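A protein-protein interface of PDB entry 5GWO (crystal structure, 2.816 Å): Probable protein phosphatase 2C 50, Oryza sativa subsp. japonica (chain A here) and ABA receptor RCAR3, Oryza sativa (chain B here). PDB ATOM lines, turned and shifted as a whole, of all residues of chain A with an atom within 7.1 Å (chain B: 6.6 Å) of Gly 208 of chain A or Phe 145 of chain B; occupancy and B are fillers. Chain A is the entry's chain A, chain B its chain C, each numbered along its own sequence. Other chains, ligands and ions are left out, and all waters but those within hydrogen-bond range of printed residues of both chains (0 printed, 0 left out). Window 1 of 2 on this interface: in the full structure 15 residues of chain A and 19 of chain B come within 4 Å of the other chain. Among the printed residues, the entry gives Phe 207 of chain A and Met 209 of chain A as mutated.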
ATOM      1  N   LYS A 197      18.350  18.707   7.443  1.00  0.00           N
ATOM      2  CA  LYS A 197      19.247  19.117   8.507  1.00  0.00           C
ATOM      3  C   LYS A 197      20.677  19.081   7.996  1.00  0.00           C
ATOM      4  O   LYS A 197      21.056  18.187   7.235  1.00  0.00           O
ATOM      5  CB  LYS A 197      19.083  18.227   9.744  1.00  0.00           C
ATOM      6  CG  LYS A 197      17.626  17.994  10.117  1.00  0.00           C
ATOM      7  CD  LYS A 197      17.432  17.829  11.621  1.00  0.00           C
ATOM      8  CE  LYS A 197      15.944  17.785  11.992  1.00  0.00           C
ATOM      9  NZ  LYS A 197      15.176  19.001  11.596  1.00  0.00           N
ATOM     10  N   VAL A 198      21.456  20.080   8.406  1.00  0.00           N
ATOM     11  CA  VAL A 198      22.877  20.175   8.098  1.00  0.00           C
ATOM     12  C   VAL A 198      23.638  19.929   9.390  1.00  0.00           C
ATOM     13  O   VAL A 198      23.509  20.702  10.350  1.00  0.00           O
ATOM     14  CB  VAL A 198      23.242  21.536   7.487  1.00  0.00           C
ATOM     15  CG1 VAL A 198      24.741  21.624   7.271  1.00  0.00           C
ATOM     16  CG2 VAL A 198      22.501  21.741   6.172  1.00  0.00           C
ATOM     17  N   ILE A 199      24.425  18.857   9.418  1.00  0.00           N
ATOM     18  CA  ILE A 199      25.119  18.404  10.618  1.00  0.00           C
ATOM     19  C   ILE A 199      26.623  18.501  10.399  1.00  0.00           C
ATOM     20  O   ILE A 199      27.133  18.094   9.350  1.00  0.00           O
ATOM     21  CB  ILE A 199      24.715  16.960  10.967  1.00  0.00           C
ATOM     22  CG1 ILE A 199      23.192  16.822  10.936  1.00  0.00           C
ATOM     23  CG2 ILE A 199      25.303  16.548  12.312  1.00  0.00           C
ATOM     24  CD1 ILE A 199      22.715  15.396  11.061  1.00  0.00           C
ATOM     25  N   GLN A 200      27.334  19.029  11.390  1.00  0.00           N
ATOM     26  CA  GLN A 200      28.792  19.034  11.323  1.00  0.00           C
ATOM     27  C   GLN A 200      29.295  17.666  11.760  1.00  0.00           C
ATOM     28  O   GLN A 200      29.358  17.365  12.952  1.00  0.00           O
ATOM     29  CB  GLN A 200      29.387  20.129  12.192  1.00  0.00           C
ATOM     30  CG  GLN A 200      30.893  20.161  12.111  1.00  0.00           C
ATOM     31  CD  GLN A 200      31.469  21.267  12.938  1.00  0.00           C
ATOM     32  OE1 GLN A 200      30.794  21.806  13.816  1.00  0.00           O
ATOM     33  NE2 GLN A 200      32.721  21.623  12.670  1.00  0.00           N
ATOM     34  N   TRP A 201      29.644  16.829  10.783  1.00  0.00           N
ATOM     35  CA  TRP A 201      30.068  15.446  11.015  1.00  0.00           C
ATOM     36  C   TRP A 201      31.270  15.192  10.109  1.00  0.00           C
ATOM     37  O   TRP A 201      31.118  14.737   8.971  1.00  0.00           O
ATOM     38  CB  TRP A 201      28.929  14.478  10.732  1.00  0.00           C
ATOM     39  CG  TRP A 201      29.038  13.166  11.449  1.00  0.00           C
ATOM     40  CD1 TRP A 201      29.876  12.138  11.145  1.00  0.00           C
ATOM     41  CD2 TRP A 201      28.241  12.724  12.556  1.00  0.00           C
ATOM     42  NE1 TRP A 201      29.666  11.086  12.006  1.00  0.00           N
ATOM     43  CE2 TRP A 201      28.665  11.420  12.880  1.00  0.00           C
ATOM     44  CE3 TRP A 201      27.215  13.307  13.309  1.00  0.00           C
ATOM     45  CZ2 TRP A 201      28.107  10.691  13.930  1.00  0.00           C
ATOM     46  CZ3 TRP A 201      26.652  12.579  14.342  1.00  0.00           C
ATOM     47  CH2 TRP A 201      27.101  11.284  14.645  1.00  0.00           C
ATOM     48  N   ASN A 202      32.463  15.488  10.613  1.00  0.00           N
ATOM     49  CA  ASN A 202      33.654  15.525   9.768  1.00  0.00           C
ATOM     50  C   ASN A 202      33.440  16.508   8.613  1.00  0.00           C
ATOM     51  O   ASN A 202      33.666  16.201   7.445  1.00  0.00           O
ATOM     52  CB  ASN A 202      34.009  14.125   9.266  1.00  0.00           C
ATOM     53  CG  ASN A 202      35.333  14.087   8.534  1.00  0.00           C
ATOM     54  OD1 ASN A 202      36.153  15.001   8.669  1.00  0.00           O
ATOM     55  ND2 ASN A 202      35.557  13.022   7.754  1.00  0.00           N
ATOM     56  N   GLY A 203      32.991  17.703   8.960  1.00  0.00           N
ATOM     57  CA  GLY A 203      32.554  18.702   8.012  1.00  0.00           C
ATOM     58  C   GLY A 203      31.043  18.875   8.042  1.00  0.00           C
ATOM     59  O   GLY A 203      30.295  18.027   8.538  1.00  0.00           O
ATOM     60  N   TYR A 204      30.592  20.004   7.507  1.00  0.00           N
ATOM     61  CA  TYR A 204      29.162  20.242   7.400  1.00  0.00           C
ATOM     62  C   TYR A 204      28.605  19.429   6.243  1.00  0.00           C
ATOM     63  O   TYR A 204      29.127  19.491   5.125  1.00  0.00           O
ATOM     64  CB  TYR A 204      28.884  21.727   7.208  1.00  0.00           C
ATOM     65  CG  TYR A 204      29.005  22.519   8.480  1.00  0.00           C
ATOM     66  CD1 TYR A 204      27.918  22.668   9.334  1.00  0.00           C
ATOM     67  CD2 TYR A 204      30.212  23.096   8.850  1.00  0.00           C
ATOM     68  CE1 TYR A 204      28.030  23.398  10.510  1.00  0.00           C
ATOM     69  CE2 TYR A 204      30.335  23.815  10.025  1.00  0.00           C
ATOM     70  CZ  TYR A 204      29.246  23.960  10.846  1.00  0.00           C
ATOM     71  OH  TYR A 204      29.360  24.683  12.000  1.00  0.00           O
ATOM     72  N   ARG A 205      27.544  18.664   6.517  1.00  0.00           N
ATOM     73  CA  ARG A 205      27.009  17.691   5.574  1.00  0.00           C
ATOM     74  C   ARG A 205      25.496  17.617   5.698  1.00  0.00           C
ATOM     75  O   ARG A 205      24.927  17.838   6.769  1.00  0.00           O
ATOM     76  CB  ARG A 205      27.580  16.284   5.809  1.00  0.00           C
ATOM     77  CG  ARG A 205      29.078  16.203   5.708  1.00  0.00           C
ATOM     78  CD  ARG A 205      29.604  14.864   6.171  1.00  0.00           C
ATOM     79  NE  ARG A 205      31.061  14.842   6.086  1.00  0.00           N
ATOM     80  CZ  ARG A 205      31.741  14.323   5.069  1.00  0.00           C
ATOM     81  NH1 ARG A 205      31.087  13.764   4.061  1.00  0.00           N
ATOM     82  NH2 ARG A 205      33.067  14.351   5.065  1.00  0.00           N
ATOM     83  N   VAL A 206      24.859  17.255   4.590  1.00  0.00           N
ATOM     84  CA  VAL A 206      23.408  17.149   4.541  1.00  0.00           C
ATOM     85  C   VAL A 206      22.991  15.828   5.172  1.00  0.00           C
ATOM     86  O   VAL A 206      23.345  14.749   4.683  1.00  0.00           O
ATOM     87  CB  VAL A 206      22.899  17.263   3.105  1.00  0.00           C
ATOM     88  CG1 VAL A 206      21.383  17.244   3.100  1.00  0.00           C
ATOM     89  CG2 VAL A 206      23.432  18.534   2.483  1.00  0.00           C
ATOM     90  N   PHE A 207      22.244  15.912   6.270  1.00  0.00           N
ATOM     91  CA  PHE A 207      21.928  14.743   7.081  1.00  0.00           C
ATOM     92  C   PHE A 207      23.197  14.060   7.565  1.00  0.00           C
ATOM     93  O   PHE A 207      23.208  12.860   7.846  1.00  0.00           O
ATOM     94  CB  PHE A 207      21.039  13.772   6.304  1.00  0.00           C
ATOM     95  CG  PHE A 207      19.590  14.114   6.394  1.00  0.00           C
ATOM     96  CD1 PHE A 207      18.857  13.750   7.517  1.00  0.00           C
ATOM     97  CD2 PHE A 207      18.974  14.855   5.400  1.00  0.00           C
ATOM     98  CE1 PHE A 207      17.524  14.079   7.630  1.00  0.00           C
ATOM     99  CE2 PHE A 207      17.639  15.193   5.506  1.00  0.00           C
ATOM    100  CZ  PHE A 207      16.913  14.804   6.627  1.00  0.00           C
ATOM    101  N   GLY A 208      24.266  14.841   7.692  1.00  0.00           N
ATOM    102  CA  GLY A 208      25.537  14.303   8.105  1.00  0.00           C
ATOM    103  C   GLY A 208      26.210  13.419   7.085  1.00  0.00           C
ATOM    104  O   GLY A 208      27.222  12.797   7.406  1.00  0.00           O
ATOM    105  N   MET A 209      25.711  13.371   5.850  1.00  0.00           N
ATOM    106  CA  MET A 209      26.219  12.439   4.850  1.00  0.00           C
ATOM    107  C   MET A 209      27.032  13.142   3.767  1.00  0.00           C
ATOM    108  O   MET A 209      28.249  12.962   3.702  1.00  0.00           O
ATOM    109  CB  MET A 209      25.050  11.654   4.258  1.00  0.00           C
ATOM    110  CG  MET A 209      24.450  10.732   5.269  1.00  0.00           C
ATOM    111  SD  MET A 209      23.109   9.728   4.644  1.00  0.00           S
ATOM    112  CE  MET A 209      21.752  10.874   4.835  1.00  0.00           C
ATOM    113  N   LEU A 210      26.407  13.967   2.940  1.00  0.00           N
ATOM    114  CA  LEU A 210      27.058  14.532   1.770  1.00  0.00           C
ATOM    115  C   LEU A 210      27.544  15.935   2.095  1.00  0.00           C
ATOM    116  O   LEU A 210      26.779  16.753   2.617  1.00  0.00           O
ATOM    117  CB  LEU A 210      26.096  14.558   0.587  1.00  0.00           C
ATOM    118  CG  LEU A 210      26.681  14.853  -0.789  1.00  0.00           C
ATOM    119  CD1 LEU A 210      27.592  13.720  -1.232  1.00  0.00           C
ATOM    120  CD2 LEU A 210      25.544  15.037  -1.764  1.00  0.00           C
ATOM    121  N   ALA A 211      28.828  16.194   1.831  1.00  0.00           N
ATOM    122  CA  ALA A 211      29.434  17.486   2.145  1.00  0.00           C
ATOM    123  C   ALA A 211      29.223  18.515   1.037  1.00  0.00           C
ATOM    124  O   ALA A 211      30.091  19.355   0.783  1.00  0.00           O
ATOM    125  CB  ALA A 211      30.920  17.309   2.421  1.00  0.00           C
ATOM    126  N   GLY B  72      31.353   9.948  -0.669  1.00  0.00           N
ATOM    127  CA  GLY B  72      30.158  10.700  -0.347  1.00  0.00           C
ATOM    128  C   GLY B  72      29.686  10.539   1.077  1.00  0.00           C
ATOM    129  O   GLY B  72      28.504  10.771   1.359  1.00  0.00           O
ATOM    130  N   LEU B  73      30.570  10.162   1.985  1.00  0.00           N
ATOM    131  CA  LEU B  73      30.215   9.921   3.373  1.00  0.00           C
ATOM    132  C   LEU B  73      31.322  10.471   4.252  1.00  0.00           C
ATOM    133  O   LEU B  73      32.441  10.708   3.784  1.00  0.00           O
ATOM    134  CB  LEU B  73      29.991   8.424   3.645  1.00  0.00           C
ATOM    135  CG  LEU B  73      28.758   7.731   3.040  1.00  0.00           C
ATOM    136  CD1 LEU B  73      28.877   6.223   3.170  1.00  0.00           C
ATOM    137  CD2 LEU B  73      27.431   8.211   3.668  1.00  0.00           C
ATOM    138  N   PRO B  74      31.047  10.680   5.542  1.00  0.00           N
ATOM    139  CA  PRO B  74      32.049  11.259   6.436  1.00  0.00           C
ATOM    140  C   PRO B  74      33.111  10.278   6.914  1.00  0.00           C
ATOM    141  O   PRO B  74      34.010  10.691   7.658  1.00  0.00           O
ATOM    142  CB  PRO B  74      31.194  11.764   7.613  1.00  0.00           C
ATOM    143  CG  PRO B  74      29.789  11.173   7.413  1.00  0.00           C
ATOM    144  CD  PRO B  74      29.858  10.226   6.281  1.00  0.00           C
ATOM    145  N   ALA B  75      33.019   8.999   6.536  1.00  0.00           N
ATOM    146  CA  ALA B  75      34.000   7.984   6.900  1.00  0.00           C
ATOM    147  C   ALA B  75      34.242   7.073   5.703  1.00  0.00           C
ATOM    148  O   ALA B  75      33.470   7.059   4.741  1.00  0.00           O
ATOM    149  CB  ALA B  75      33.548   7.159   8.113  1.00  0.00           C
ATOM    150  N   LEU B 103      31.171   6.728  15.414  1.00  0.00           N
ATOM    151  CA  LEU B 103      30.115   5.979  16.096  1.00  0.00           C
ATOM    152  C   LEU B 103      30.778   4.967  17.027  1.00  0.00           C
ATOM    153  O   LEU B 103      30.796   3.767  16.750  1.00  0.00           O
ATOM    154  CB  LEU B 103      29.212   5.306  15.099  1.00  0.00           C
ATOM    155  CG  LEU B 103      28.422   6.200  14.151  1.00  0.00           C
ATOM    156  CD1 LEU B 103      27.557   5.343  13.262  1.00  0.00           C
ATOM    157  CD2 LEU B 103      27.576   7.190  14.927  1.00  0.00           C
ATOM    158  N   ASP B 140      20.145  14.430  19.037  1.00  0.00           N
ATOM    159  CA  ASP B 140      19.274  14.501  17.867  1.00  0.00           C
ATOM    160  C   ASP B 140      20.075  14.387  16.577  1.00  0.00           C
ATOM    161  O   ASP B 140      19.701  13.636  15.674  1.00  0.00           O
ATOM    162  CB  ASP B 140      18.450  15.786  17.892  1.00  0.00           C
ATOM    163  CG  ASP B 140      17.365  15.755  18.956  1.00  0.00           C
ATOM    164  OD1 ASP B 140      17.582  15.106  20.004  1.00  0.00           O
ATOM    165  OD2 ASP B 140      16.292  16.363  18.744  1.00  0.00           O
ATOM    166  N   GLU B 141      21.184  15.123  16.472  1.00  0.00           N
ATOM    167  CA  GLU B 141      22.037  15.024  15.284  1.00  0.00           C
ATOM    168  C   GLU B 141      22.485  13.586  15.050  1.00  0.00           C
ATOM    169  O   GLU B 141      22.373  13.055  13.935  1.00  0.00           O
ATOM    170  CB  GLU B 141      23.242  15.942  15.436  1.00  0.00           C
ATOM    171  CG  GLU B 141      22.897  17.414  15.400  1.00  0.00           C
ATOM    172  CD  GLU B 141      24.118  18.299  15.574  1.00  0.00           C
ATOM    173  OE1 GLU B 141      24.943  17.978  16.463  1.00  0.00           O
ATOM    174  OE2 GLU B 141      24.253  19.299  14.821  1.00  0.00           O
ATOM    175  N   THR B 142      23.003  12.943  16.096  1.00  0.00           N
ATOM    176  CA  THR B 142      23.415  11.548  15.989  1.00  0.00           C
ATOM    177  C   THR B 142      22.281  10.684  15.458  1.00  0.00           C
ATOM    178  O   THR B 142      22.479   9.857  14.561  1.00  0.00           O
ATOM    179  CB  THR B 142      23.859  11.027  17.351  1.00  0.00           C
ATOM    180  OG1 THR B 142      24.836  11.911  17.917  1.00  0.00           O
ATOM    181  CG2 THR B 142      24.453   9.641  17.194  1.00  0.00           C
ATOM    182  N   CYS B 143      21.078  10.856  16.014  1.00  0.00           N
ATOM    183  CA  CYS B 143      19.957  10.019  15.593  1.00  0.00           C
ATOM    184  C   CYS B 143      19.544  10.289  14.146  1.00  0.00           C
ATOM    185  O   CYS B 143      19.249   9.349  13.407  1.00  0.00           O
ATOM    186  CB  CYS B 143      18.784  10.185  16.553  1.00  0.00           C
ATOM    187  SG  CYS B 143      19.052   9.316  18.111  1.00  0.00           S
ATOM    188  N   TYR B 144      19.509  11.555  13.718  1.00  0.00           N
ATOM    189  CA  TYR B 144      19.170  11.836  12.327  1.00  0.00           C
ATOM    190  C   TYR B 144      20.188  11.216  11.383  1.00  0.00           C
ATOM    191  O   TYR B 144      19.828  10.710  10.312  1.00  0.00           O
ATOM    192  CB  TYR B 144      19.068  13.346  12.087  1.00  0.00           C
ATOM    193  CG  TYR B 144      17.778  13.954  12.588  1.00  0.00           C
ATOM    194  CD1 TYR B 144      16.566  13.665  11.969  1.00  0.00           C
ATOM    195  CD2 TYR B 144      17.765  14.810  13.682  1.00  0.00           C
ATOM    196  CE1 TYR B 144      15.377  14.212  12.423  1.00  0.00           C
ATOM    197  CE2 TYR B 144      16.579  15.363  14.146  1.00  0.00           C
ATOM    198  CZ  TYR B 144      15.390  15.060  13.513  1.00  0.00           C
ATOM    199  OH  TYR B 144      14.211  15.608  13.967  1.00  0.00           O
ATOM    200  N   PHE B 145      21.466  11.247  11.759  1.00  0.00           N
ATOM    201  CA  PHE B 145      22.496  10.619  10.939  1.00  0.00           C
ATOM    202  C   PHE B 145      22.269   9.112  10.834  1.00  0.00           C
ATOM    203  O   PHE B 145      22.098   8.561   9.735  1.00  0.00           O
ATOM    204  CB  PHE B 145      23.873  10.937  11.531  1.00  0.00           C
ATOM    205  CG  PHE B 145      25.026  10.406  10.727  1.00  0.00           C
ATOM    206  CD1 PHE B 145      25.180  10.747   9.397  1.00  0.00           C
ATOM    207  CD2 PHE B 145      25.957   9.566  11.300  1.00  0.00           C
ATOM    208  CE1 PHE B 145      26.247  10.263   8.657  1.00  0.00           C
ATOM    209  CE2 PHE B 145      27.023   9.075  10.558  1.00  0.00           C
ATOM    210  CZ  PHE B 145      27.170   9.426   9.243  1.00  0.00           C
ATOM    211  N   VAL B 146      22.250   8.425  11.982  1.00  0.00           N
ATOM    212  CA  VAL B 146      22.118   6.972  11.973  1.00  0.00           C
ATOM    213  C   VAL B 146      20.816   6.548  11.316  1.00  0.00           C
ATOM    214  O   VAL B 146      20.757   5.512  10.642  1.00  0.00           O
ATOM    215  CB  VAL B 146      22.240   6.411  13.398  1.00  0.00           C
ATOM    216  CG1 VAL B 146      22.084   4.911  13.384  1.00  0.00           C
ATOM    217  CG2 VAL B 146      23.594   6.749  13.961  1.00  0.00           C
ATOM    218  N   GLU B 147      19.746   7.315  11.528  1.00  0.00           N
ATOM    219  CA  GLU B 147      18.457   6.964  10.938  1.00  0.00           C
ATOM    220  C   GLU B 147      18.470   7.157   9.430  1.00  0.00           C
ATOM    221  O   GLU B 147      17.943   6.322   8.695  1.00  0.00           O
ATOM    222  CB  GLU B 147      17.339   7.785  11.575  1.00  0.00           C
ATOM    223  CG  GLU B 147      17.022   7.434  13.018  1.00  0.00           C
ATOM    224  CD  GLU B 147      16.179   8.506  13.679  1.00  0.00           C
ATOM    225  OE1 GLU B 147      15.831   9.487  12.985  1.00  0.00           O
ATOM    226  OE2 GLU B 147      15.873   8.382  14.884  1.00  0.00           O
ATOM    227  N   ALA B 148      19.087   8.238   8.943  1.00  0.00           N
ATOM    228  CA  ALA B 148      19.238   8.387   7.501  1.00  0.00           C
ATOM    229  C   ALA B 148      19.961   7.180   6.916  1.00  0.00           C
ATOM    230  O   ALA B 148      19.490   6.557   5.948  1.00  0.00           O
ATOM    231  CB  ALA B 148      19.982   9.681   7.179  1.00  0.00           C
ATOM    232  N   LEU B 149      21.099   6.813   7.514  1.00  0.00           N
ATOM    233  CA  LEU B 149      21.857   5.672   7.003  1.00  0.00           C
ATOM    234  C   LEU B 149      21.039   4.382   7.032  1.00  0.00           C
ATOM    235  O   LEU B 149      20.975   3.652   6.033  1.00  0.00           O
ATOM    236  CB  LEU B 149      23.140   5.499   7.800  1.00  0.00           C
ATOM    237  CG  LEU B 149      24.165   6.564   7.456  1.00  0.00           C
ATOM    238  CD1 LEU B 149      25.454   6.315   8.246  1.00  0.00           C
ATOM    239  CD2 LEU B 149      24.396   6.572   5.947  1.00  0.00           C
ATOM    240  N   LEU B 150      20.422   4.069   8.174  1.00  0.00           N
ATOM    241  CA  LEU B 150      19.674   2.821   8.272  1.00  0.00           C
ATOM    242  C   LEU B 150      18.470   2.806   7.331  1.00  0.00           C
ATOM    243  O   LEU B 150      18.132   1.752   6.783  1.00  0.00           O
ATOM    244  CB  LEU B 150      19.252   2.571   9.729  1.00  0.00           C
ATOM    245  CG  LEU B 150      20.357   2.238  10.754  1.00  0.00           C
ATOM    246  CD1 LEU B 150      19.793   2.006  12.141  1.00  0.00           C
ATOM    247  CD2 LEU B 150      21.154   1.014  10.328  1.00  0.00           C
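O of Pro 74 of chain B is in hydrogen-bond range of ND2 of Asn 202 of chain A (2.8 Å).
NH1 of Arg 205 of chain A lies close to O of Leu 73 of chain B (3.4 Å).
The guanidinium group (NH1) of Arg 205 of chain A lies close to the backbone nitrogen (N) of Pro 74 of chain B (3.4 Å).
The backbone carbonyl oxygen of Gly 72 of chain B sits close to the backbone carbonyl oxygen of Met 209 of chain A, 3.2 Å away.
N of Phe 207 of chain A is in hydrogen-bond range of O of Lys 197 of chain A (2.7 Å).
O of Arg 205 of chain A sits at hydrogen-bond distance from N of Ile 199 of chain A (2.9 Å).
The guanidinium group of Arg 205 of chain A lies within hydrogen-bond range of the backbone carbonyl oxygen of Trp 201 of chain A (2.9 Å).
The backbone carbonyl oxygen of Asn 202 of chain A lies within hydrogen-bond range of the guanidinium group of Arg 205 of chain A.
The backbone carbonyl oxygen of Met 209 of chain A lies within hydrogen-bond range of the guanidinium group of Arg 205 of chain A (3.0 Å).
Lys 197 of chain A touches Tyr 144 of chain B.
O of Glu 141 of chain B touches CD1 of Ile 199 of chain A (3.7 Å).
Trp 201 of chain A touches Leu 103 of chain B (CZ2 to CD2, 3.7 Å).
Thr 142 of chain B touches Trp 201 of chain A (CA to CZ3, 3.8 Å).
CD2 of Phe 145 of chain B touches CZ2 of Trp 201 of chain A, at 3.6 Å.
O of Phe 207 of chain A touches CD1 of Phe 145 of chain B (3.3 Å).
Pro 74 of chain B touches Gly 208 of chain A (CG to O, 3.0 Å).
Gly 208 of chain A touches Phe 145 of chain B.
CB of Ala 148 of chain B touches CE of Met 209 of chain A (3.2 Å).
Leu 149 of chain B touches Met 209 of chain A (CD2 to SD, 3.6 Å).
Of chain B, only Pro 74 and Phe 145 come within 4 Å of Gly 208 of chain A.
Phe 145 of chain B touches just these residues of chain A: Trp 201, Phe 207, Gly 208 and Met 209.
Of the printed residues of chain B, Ile 199 of chain A touches Glu 141 (3.7 Å).
Printed residues of chain B within 4 Å of Lys 197 of chain A: Tyr 144.
Printed residues of chain B within 4 Å of Arg 205 of chain A: Leu 73 and Pro 74.
Of the printed residues of chain A, Glu 141 of chain B touches Ile 199 (3.7 Å).
Of the printed residues of chain A, Leu 103 of chain B touches Trp 201 (3.7 Å).
Gly 203 of chain A touches none of the printed residues of chain B.
The nearest residue of chain B that does not touch Gly 208 of chain A is Leu 73 of chain B (5.7 Å).
Of the 15 printed residues of chain A, 8 touch a printed residue of chain B.
Hydrophobic or aromatic side chains of chain A that line the printed part of chain B: Ile 199, Trp 201 and Met 209.
Printed residues of chain B that touch a printed residue of chain A: Gly 72, Leu 73, Pro 74, Leu 103, Glu 141, Thr 142, Tyr 144, Phe 145, Ala 148 and Leu 149.
Hydrophobic or aromatic side chains of chain B that line the printed part of chain A: Pro 74, Leu 103, Tyr 144, Phe 145, Ala 148 and Leu 149.
Among the printed residues, no Asp or Glu carboxylate lies within 4 Å of a Lys or Arg side-chain nitrogen of the other chain.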
